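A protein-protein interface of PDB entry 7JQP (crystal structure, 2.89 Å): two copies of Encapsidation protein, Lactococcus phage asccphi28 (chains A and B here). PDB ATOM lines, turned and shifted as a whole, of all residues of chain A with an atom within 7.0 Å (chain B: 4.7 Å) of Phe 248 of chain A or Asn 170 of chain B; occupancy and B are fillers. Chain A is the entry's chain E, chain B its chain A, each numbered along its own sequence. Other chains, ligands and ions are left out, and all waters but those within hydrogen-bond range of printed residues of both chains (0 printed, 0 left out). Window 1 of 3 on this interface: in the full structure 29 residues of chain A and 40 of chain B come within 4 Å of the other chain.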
ATOM      1  N   ARG A  28       5.760 -13.275 -22.932  1.00  0.00           N
ATOM      2  CA  ARG A  28       4.891 -12.267 -22.346  1.00  0.00           C
ATOM      3  C   ARG A  28       5.316 -10.879 -22.808  1.00  0.00           C
ATOM      4  O   ARG A  28       6.508 -10.564 -22.874  1.00  0.00           O
ATOM      5  CB  ARG A  28       4.942 -12.334 -20.820  1.00  0.00           C
ATOM      6  CG  ARG A  28       4.538 -13.661 -20.211  1.00  0.00           C
ATOM      7  CD  ARG A  28       4.781 -13.647 -18.703  1.00  0.00           C
ATOM      8  NE  ARG A  28       4.404 -12.366 -18.109  1.00  0.00           N
ATOM      9  CZ  ARG A  28       3.195 -12.081 -17.636  1.00  0.00           C
ATOM     10  NH1 ARG A  28       2.222 -12.986 -17.674  1.00  0.00           N
ATOM     11  NH2 ARG A  28       2.955 -10.882 -17.120  1.00  0.00           N
ATOM     12  N   SER A 153      -0.547 -16.172 -10.911  1.00  0.00           N
ATOM     13  CA  SER A 153       0.010 -14.939 -10.358  1.00  0.00           C
ATOM     14  C   SER A 153      -0.867 -13.734 -10.721  1.00  0.00           C
ATOM     15  O   SER A 153      -1.321 -13.008  -9.832  1.00  0.00           O
ATOM     16  CB  SER A 153       1.436 -14.736 -10.892  1.00  0.00           C
ATOM     17  OG  SER A 153       2.258 -15.835 -10.506  1.00  0.00           O
ATOM     18  N   ILE A 154      -1.171 -13.530 -12.016  1.00  0.00           N
ATOM     19  CA  ILE A 154      -2.004 -12.392 -12.414  1.00  0.00           C
ATOM     20  C   ILE A 154      -3.439 -12.617 -11.948  1.00  0.00           C
ATOM     21  O   ILE A 154      -4.078 -11.727 -11.373  1.00  0.00           O
ATOM     22  CB  ILE A 154      -1.936 -12.199 -13.939  1.00  0.00           C
ATOM     23  CG1 ILE A 154      -0.513 -11.816 -14.368  1.00  0.00           C
ATOM     24  CG2 ILE A 154      -2.950 -11.116 -14.378  1.00  0.00           C
ATOM     25  CD1 ILE A 154      -0.287 -11.796 -15.887  1.00  0.00           C
ATOM     26  N   PHE A 238       9.300   4.096 -14.237  1.00  0.00           N
ATOM     27  CA  PHE A 238       8.370   2.972 -14.175  1.00  0.00           C
ATOM     28  C   PHE A 238       9.096   1.638 -14.279  1.00  0.00           C
ATOM     29  O   PHE A 238       8.744   0.674 -13.588  1.00  0.00           O
ATOM     30  CB  PHE A 238       7.327   3.099 -15.285  1.00  0.00           C
ATOM     31  CG  PHE A 238       6.374   4.239 -15.090  1.00  0.00           C
ATOM     32  CD1 PHE A 238       5.260   4.092 -14.283  1.00  0.00           C
ATOM     33  CD2 PHE A 238       6.594   5.459 -15.707  1.00  0.00           C
ATOM     34  CE1 PHE A 238       4.378   5.140 -14.098  1.00  0.00           C
ATOM     35  CE2 PHE A 238       5.718   6.511 -15.525  1.00  0.00           C
ATOM     36  CZ  PHE A 238       4.610   6.351 -14.718  1.00  0.00           C
ATOM     37  N   VAL A 239      10.114   1.561 -15.135  1.00  0.00           N
ATOM     38  CA  VAL A 239      10.873   0.322 -15.261  1.00  0.00           C
ATOM     39  C   VAL A 239      11.630   0.030 -13.972  1.00  0.00           C
ATOM     40  O   VAL A 239      11.692  -1.121 -13.522  1.00  0.00           O
ATOM     41  CB  VAL A 239      11.816   0.399 -16.474  1.00  0.00           C
ATOM     42  CG1 VAL A 239      12.709  -0.824 -16.527  1.00  0.00           C
ATOM     43  CG2 VAL A 239      11.011   0.529 -17.757  1.00  0.00           C
ATOM     44  N   LEU A 241      10.804   0.887 -10.929  1.00  0.00           N
ATOM     45  CA  LEU A 241       9.870   0.453  -9.895  1.00  0.00           C
ATOM     46  C   LEU A 241       9.505  -1.017 -10.058  1.00  0.00           C
ATOM     47  O   LEU A 241       9.422  -1.757  -9.070  1.00  0.00           O
ATOM     48  CB  LEU A 241       8.610   1.318  -9.924  1.00  0.00           C
ATOM     49  CG  LEU A 241       7.580   0.999  -8.839  1.00  0.00           C
ATOM     50  CD1 LEU A 241       8.137   1.331  -7.461  1.00  0.00           C
ATOM     51  CD2 LEU A 241       6.276   1.740  -9.088  1.00  0.00           C
ATOM     52  N   GLY A 242       9.275  -1.456 -11.297  1.00  0.00           N
ATOM     53  CA  GLY A 242       8.944  -2.853 -11.522  1.00  0.00           C
ATOM     54  C   GLY A 242      10.075  -3.787 -11.137  1.00  0.00           C
ATOM     55  O   GLY A 242       9.845  -4.853 -10.559  1.00  0.00           O
ATOM     56  N   ALA A 243      11.311  -3.402 -11.453  1.00  0.00           N
ATOM     57  CA  ALA A 243      12.451  -4.239 -11.098  1.00  0.00           C
ATOM     58  C   ALA A 243      12.564  -4.401  -9.588  1.00  0.00           C
ATOM     59  O   ALA A 243      12.945  -5.470  -9.098  1.00  0.00           O
ATOM     60  CB  ALA A 243      13.738  -3.642 -11.671  1.00  0.00           C
ATOM     61  N   LYS A 244      12.236  -3.350  -8.830  1.00  0.00           N
ATOM     62  CA  LYS A 244      12.335  -3.453  -7.380  1.00  0.00           C
ATOM     63  C   LYS A 244      11.335  -4.455  -6.810  1.00  0.00           C
ATOM     64  O   LYS A 244      11.619  -5.095  -5.792  1.00  0.00           O
ATOM     65  CB  LYS A 244      12.150  -2.084  -6.722  1.00  0.00           C
ATOM     66  CG  LYS A 244      13.287  -1.127  -7.040  1.00  0.00           C
ATOM     67  CD  LYS A 244      13.199   0.173  -6.263  1.00  0.00           C
ATOM     68  CE  LYS A 244      14.348   1.095  -6.646  1.00  0.00           C
ATOM     69  NZ  LYS A 244      14.538   2.207  -5.678  1.00  0.00           N
ATOM     70  N   ASN A 245      10.171  -4.602  -7.431  1.00  0.00           N
ATOM     71  CA  ASN A 245       9.178  -5.584  -7.004  1.00  0.00           C
ATOM     72  C   ASN A 245       9.518  -6.924  -7.648  1.00  0.00           C
ATOM     73  O   ASN A 245       9.346  -7.099  -8.857  1.00  0.00           O
ATOM     74  CB  ASN A 245       7.772  -5.129  -7.379  1.00  0.00           C
ATOM     75  CG  ASN A 245       7.213  -4.120  -6.403  1.00  0.00           C
ATOM     76  OD1 ASN A 245       6.385  -4.452  -5.555  1.00  0.00           O
ATOM     77  ND2 ASN A 245       7.667  -2.875  -6.513  1.00  0.00           N
ATOM     78  N   ARG A 246       9.994  -7.873  -6.838  1.00  0.00           N
ATOM     79  CA  ARG A 246      10.443  -9.145  -7.394  1.00  0.00           C
ATOM     80  C   ARG A 246       9.276  -9.961  -7.935  1.00  0.00           C
ATOM     81  O   ARG A 246       9.392 -10.594  -8.992  1.00  0.00           O
ATOM     82  CB  ARG A 246      11.187  -9.953  -6.335  1.00  0.00           C
ATOM     83  CG  ARG A 246      11.694 -11.308  -6.806  1.00  0.00           C
ATOM     84  CD  ARG A 246      12.670 -11.162  -7.961  1.00  0.00           C
ATOM     85  NE  ARG A 246      13.809 -10.357  -7.530  1.00  0.00           N
ATOM     86  CZ  ARG A 246      14.832 -10.831  -6.830  1.00  0.00           C
ATOM     87  NH1 ARG A 246      14.848 -12.103  -6.459  1.00  0.00           N
ATOM     88  NH2 ARG A 246      15.824 -10.026  -6.471  1.00  0.00           N
ATOM     89  N   ASP A 247       8.144  -9.970  -7.226  1.00  0.00           N
ATOM     90  CA  ASP A 247       7.018 -10.789  -7.665  1.00  0.00           C
ATOM     91  C   ASP A 247       6.612 -10.406  -9.082  1.00  0.00           C
ATOM     92  O   ASP A 247       6.390 -11.271  -9.937  1.00  0.00           O
ATOM     93  CB  ASP A 247       5.840 -10.640  -6.704  1.00  0.00           C
ATOM     94  CG  ASP A 247       4.733 -11.652  -6.975  1.00  0.00           C
ATOM     95  OD1 ASP A 247       4.511 -12.006  -8.153  1.00  0.00           O
ATOM     96  OD2 ASP A 247       4.085 -12.096  -6.006  1.00  0.00           O
ATOM     97  N   PHE A 248       6.512  -9.104  -9.348  1.00  0.00           N
ATOM     98  CA  PHE A 248       6.222  -8.655 -10.704  1.00  0.00           C
ATOM     99  C   PHE A 248       7.373  -8.994 -11.643  1.00  0.00           C
ATOM    100  O   PHE A 248       7.150  -9.451 -12.770  1.00  0.00           O
ATOM    101  CB  PHE A 248       5.944  -7.154 -10.711  1.00  0.00           C
ATOM    102  CG  PHE A 248       5.894  -6.558 -12.084  1.00  0.00           C
ATOM    103  CD1 PHE A 248       4.773  -6.716 -12.878  1.00  0.00           C
ATOM    104  CD2 PHE A 248       6.965  -5.837 -12.579  1.00  0.00           C
ATOM    105  CE1 PHE A 248       4.724  -6.172 -14.142  1.00  0.00           C
ATOM    106  CE2 PHE A 248       6.922  -5.289 -13.842  1.00  0.00           C
ATOM    107  CZ  PHE A 248       5.800  -5.456 -14.625  1.00  0.00           C
ATOM    108  N   SER A 249       8.612  -8.782 -11.192  1.00  0.00           N
ATOM    109  CA  SER A 249       9.766  -9.058 -12.040  1.00  0.00           C
ATOM    110  C   SER A 249       9.858 -10.538 -12.380  1.00  0.00           C
ATOM    111  O   SER A 249      10.158 -10.904 -13.523  1.00  0.00           O
ATOM    112  CB  SER A 249      11.047  -8.586 -11.352  1.00  0.00           C
ATOM    113  OG  SER A 249      11.136  -7.173 -11.360  1.00  0.00           O
ATOM    114  N   ASN A 250       9.606 -11.407 -11.399  1.00  0.00           N
ATOM    115  CA  ASN A 250       9.630 -12.839 -11.669  1.00  0.00           C
ATOM    116  C   ASN A 250       8.556 -13.226 -12.677  1.00  0.00           C
ATOM    117  O   ASN A 250       8.762 -14.135 -13.487  1.00  0.00           O
ATOM    118  CB  ASN A 250       9.431 -13.621 -10.369  1.00  0.00           C
ATOM    119  CG  ASN A 250      10.718 -13.796  -9.587  1.00  0.00           C
ATOM    120  OD1 ASN A 250      11.776 -13.316  -9.994  1.00  0.00           O
ATOM    121  ND2 ASN A 250      10.633 -14.487  -8.457  1.00  0.00           N
ATOM    122  N   SER A 251       7.409 -12.541 -12.640  1.00  0.00           N
ATOM    123  CA  SER A 251       6.299 -12.881 -13.525  1.00  0.00           C
ATOM    124  C   SER A 251       6.706 -12.814 -14.992  1.00  0.00           C
ATOM    125  O   SER A 251       6.220 -13.602 -15.811  1.00  0.00           O
ATOM    126  CB  SER A 251       5.114 -11.954 -13.253  1.00  0.00           C
ATOM    127  OG  SER A 251       4.005 -12.294 -14.066  1.00  0.00           O
ATOM    128  N   LYS A 252       7.564 -11.859 -15.354  1.00  0.00           N
ATOM    129  CA  LYS A 252       7.957 -11.717 -16.754  1.00  0.00           C
ATOM    130  C   LYS A 252       8.581 -12.999 -17.289  1.00  0.00           C
ATOM    131  O   LYS A 252       8.316 -13.395 -18.429  1.00  0.00           O
ATOM    132  CB  LYS A 252       8.920 -10.541 -16.890  1.00  0.00           C
ATOM    133  CG  LYS A 252       8.279  -9.193 -16.607  1.00  0.00           C
ATOM    134  CD  LYS A 252       9.314  -8.145 -16.249  1.00  0.00           C
ATOM    135  CE  LYS A 252       8.745  -6.739 -16.312  1.00  0.00           C
ATOM    136  NZ  LYS A 252       8.812  -6.194 -17.703  1.00  0.00           N
ATOM    137  N   THR A 253       9.412 -13.660 -16.484  1.00  0.00           N
ATOM    138  CA  THR A 253      10.077 -14.894 -16.884  1.00  0.00           C
ATOM    139  C   THR A 253       9.461 -16.123 -16.221  1.00  0.00           C
ATOM    140  O   THR A 253      10.100 -17.179 -16.164  1.00  0.00           O
ATOM    141  CB  THR A 253      11.573 -14.814 -16.577  1.00  0.00           C
ATOM    142  OG1 THR A 253      11.779 -14.853 -15.160  1.00  0.00           O
ATOM    143  CG2 THR A 253      12.163 -13.525 -17.139  1.00  0.00           C
ATOM    144  N   THR B 166       1.351  -6.234  -7.826  1.00  0.00           N
ATOM    145  CA  THR B 166       1.703  -6.917  -9.065  1.00  0.00           C
ATOM    146  C   THR B 166       0.624  -6.698 -10.116  1.00  0.00           C
ATOM    147  O   THR B 166       0.926  -6.491 -11.297  1.00  0.00           O
ATOM    148  CB  THR B 166       1.917  -8.409  -8.813  1.00  0.00           C
ATOM    149  OG1 THR B 166       2.994  -8.590  -7.886  1.00  0.00           O
ATOM    150  CG2 THR B 166       2.248  -9.127 -10.114  1.00  0.00           C
ATOM    151  N   VAL B 167      -0.644  -6.734  -9.701  1.00  0.00           N
ATOM    152  CA  VAL B 167      -1.734  -6.442 -10.626  1.00  0.00           C
ATOM    153  C   VAL B 167      -1.648  -4.998 -11.101  1.00  0.00           C
ATOM    154  O   VAL B 167      -1.879  -4.700 -12.279  1.00  0.00           O
ATOM    155  CB  VAL B 167      -3.091  -6.740  -9.961  1.00  0.00           C
ATOM    156  CG1 VAL B 167      -4.238  -6.338 -10.879  1.00  0.00           C
ATOM    157  CG2 VAL B 167      -3.188  -8.215  -9.594  1.00  0.00           C
ATOM    158  N   LEU B 168      -1.302  -4.081 -10.196  1.00  0.00           N
ATOM    159  CA  LEU B 168      -1.165  -2.681 -10.579  1.00  0.00           C
ATOM    160  C   LEU B 168      -0.029  -2.495 -11.577  1.00  0.00           C
ATOM    161  O   LEU B 168      -0.203  -1.848 -12.617  1.00  0.00           O
ATOM    162  CB  LEU B 168      -0.936  -1.823  -9.334  1.00  0.00           C
ATOM    163  CG  LEU B 168      -0.662  -0.336  -9.555  1.00  0.00           C
ATOM    164  CD1 LEU B 168      -1.634   0.272 -10.547  1.00  0.00           C
ATOM    165  CD2 LEU B 168      -0.726   0.405  -8.223  1.00  0.00           C
ATOM    166  N   LEU B 169       1.142  -3.061 -11.283  1.00  0.00           N
ATOM    167  CA  LEU B 169       2.284  -2.895 -12.177  1.00  0.00           C
ATOM    168  C   LEU B 169       1.996  -3.483 -13.554  1.00  0.00           C
ATOM    169  O   LEU B 169       2.398  -2.914 -14.576  1.00  0.00           O
ATOM    170  CB  LEU B 169       3.526  -3.541 -11.567  1.00  0.00           C
ATOM    171  CG  LEU B 169       4.157  -2.815 -10.378  1.00  0.00           C
ATOM    172  CD1 LEU B 169       5.323  -3.627  -9.823  1.00  0.00           C
ATOM    173  CD2 LEU B 169       4.620  -1.417 -10.757  1.00  0.00           C
ATOM    174  N   ASN B 170       1.306  -4.624 -13.600  1.00  0.00           N
ATOM    175  CA  ASN B 170       0.922  -5.197 -14.886  1.00  0.00           C
ATOM    176  C   ASN B 170       0.002  -4.257 -15.656  1.00  0.00           C
ATOM    177  O   ASN B 170       0.119  -4.128 -16.881  1.00  0.00           O
ATOM    178  CB  ASN B 170       0.252  -6.553 -14.680  1.00  0.00           C
ATOM    179  CG  ASN B 170       1.255  -7.672 -14.481  1.00  0.00           C
ATOM    180  OD1 ASN B 170       1.312  -8.288 -13.418  1.00  0.00           O
ATOM    181  ND2 ASN B 170       2.060  -7.934 -15.506  1.00  0.00           N
ATOM    182  N   LEU B 171      -0.922  -3.592 -14.958  1.00  0.00           N
ATOM    183  CA  LEU B 171      -1.813  -2.652 -15.630  1.00  0.00           C
ATOM    184  C   LEU B 171      -1.035  -1.466 -16.185  1.00  0.00           C
ATOM    185  O   LEU B 171      -1.357  -0.956 -17.265  1.00  0.00           O
ATOM    186  CB  LEU B 171      -2.901  -2.180 -14.666  1.00  0.00           C
ATOM    187  CG  LEU B 171      -4.075  -1.415 -15.278  1.00  0.00           C
ATOM    188  CD1 LEU B 171      -4.779  -2.251 -16.338  1.00  0.00           C
ATOM    189  CD2 LEU B 171      -5.061  -0.985 -14.201  1.00  0.00           C
ATOM    190  N   ILE B 172      -0.006  -1.014 -15.464  1.00  0.00           N
ATOM    191  CA  ILE B 172       0.843   0.059 -15.974  1.00  0.00           C
ATOM    192  C   ILE B 172       1.460  -0.355 -17.304  1.00  0.00           C
ATOM    193  O   ILE B 172       1.520   0.433 -18.255  1.00  0.00           O
ATOM    194  CB  ILE B 172       1.931   0.422 -14.946  1.00  0.00           C
ATOM    195  CG1 ILE B 172       1.320   0.788 -13.593  1.00  0.00           C
ATOM    196  CG2 ILE B 172       2.790   1.568 -15.473  1.00  0.00           C
ATOM    197  CD1 ILE B 172       0.787   2.192 -13.516  1.00  0.00           C
ATOM    198  N   GLU B 173       1.924  -1.603 -17.390  1.00  0.00           N
ATOM    199  CA  GLU B 173       2.525  -2.087 -18.626  1.00  0.00           C
ATOM    200  C   GLU B 173       1.499  -2.123 -19.752  1.00  0.00           C
ATOM    201  O   GLU B 173       1.796  -1.738 -20.888  1.00  0.00           O
ATOM    202  CB  GLU B 173       3.113  -3.482 -18.406  1.00  0.00           C
ATOM    203  CG  GLU B 173       4.114  -3.913 -19.461  1.00  0.00           C
ATOM    204  CD  GLU B 173       4.335  -5.414 -19.474  1.00  0.00           C
ATOM    205  OE1 GLU B 173       3.525  -6.139 -18.857  1.00  0.00           O
ATOM    206  OE2 GLU B 173       5.309  -5.872 -20.107  1.00  0.00           O
ATOM    207  N   THR B 174       0.282  -2.586 -19.455  1.00  0.00           N
ATOM    208  CA  THR B 174      -0.754  -2.659 -20.479  1.00  0.00           C
ATOM    209  C   THR B 174      -1.155  -1.265 -20.948  1.00  0.00           C
ATOM    210  O   THR B 174      -1.288  -1.017 -22.153  1.00  0.00           O
ATOM    211  CB  THR B 174      -1.973  -3.410 -19.942  1.00  0.00           C
ATOM    212  OG1 THR B 174      -1.574  -4.696 -19.451  1.00  0.00           O
ATOM    213  CG2 THR B 174      -3.017  -3.586 -21.033  1.00  0.00           C
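The guanidinium group (NH2) of Arg 28 of chain A lies close to the side-chain amide nitrogen (ND2) of Asn 170 of chain B (3.5 Å).
O of Thr 166 of chain B sits close to OD1 of Asn 170 of chain B (2.8 Å). The backbone carbonyl oxygen (O) of Asn 170 of chain B lies within hydrogen-bond range of the side-chain hydroxyl (OG1) of Thr 174 of chain B, at 3.1 Å. The guanidinium group (NE) of Arg 28 of chain A sits at hydrogen-bond distance from the backbone carbonyl oxygen (O) of Ser 251 of chain A, 3.2 Å away. O of Leu 241 of chain A lies within hydrogen-bond range of ND2 of Asn 245 of chain A (3.3 Å). The backbone carbonyl oxygen (O) of Asn 245 of chain A is in hydrogen-bond range of the side-chain hydroxyl (OG) of Ser 249 of chain A.
Among the printed residues, merely in contact across the chains: Phe 248 of chain A with Asn 170 of chain B (3.5 Å), Asp 247 of chain A with Thr 166 of chain B (3.6 Å), Phe 248 of chain A with Leu 169 of chain B (3.7 Å), Phe 238 of chain A with Ile 172 of chain B (3.7 Å), Asn 245 of chain A with Leu 169 of chain B (3.8 Å), Phe 248 of chain A with Thr 166 of chain B (3.8 Å) and Leu 241 of chain A with Leu 169 of chain B (3.9 Å).
Of the printed residues of chain B, Leu 241 of chain A touches Leu 169 (3.9 Å). Printed residues of chain B within 4 Å of Asp 247 of chain A: Thr 166 (3.6 Å). Of chain B, only Thr 166 (3.8 Å), Leu 169 (3.7 Å) and Asn 170 (3.5 Å) come within 4 Å of Phe 248 of chain A. Of the printed residues of chain A, Thr 166 of chain B touches Asp 247 and Phe 248. Printed residues of chain A within 4 Å of Leu 169 of chain B: Leu 241 (3.9 Å), Asn 245 (3.8 Å) and Phe 248 (3.7 Å). Asn 170 of chain B touches just these residues of chain A: Arg 28 (3.5 Å) and Phe 248 (3.5 Å). Of the printed residues of chain A, Ile 172 of chain B touches Phe 238 (3.7 Å). The nearest printed residue of chain A that does not touch Ile 172 of chain B is Leu 241 of chain A (6.8 Å).
Hydrophobic or aromatic side chains of chain B that line the printed part of chain A: Leu 169 and Ile 172. Printed residues of chain A that touch a printed residue of chain B: Arg 28, Phe 238, Leu 241, Asn 245, Asp 247 and Phe 248. Hydrophobic or aromatic side chains of chain A within 4 Å of the printed part of chain B: Phe 238, Leu 241 and Phe 248. Among the printed residues, no Asp or Glu carboxylate lies within 4 Å of a Lys or Arg side-chain nitrogen of the other chain.
No position is printed for both chains.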
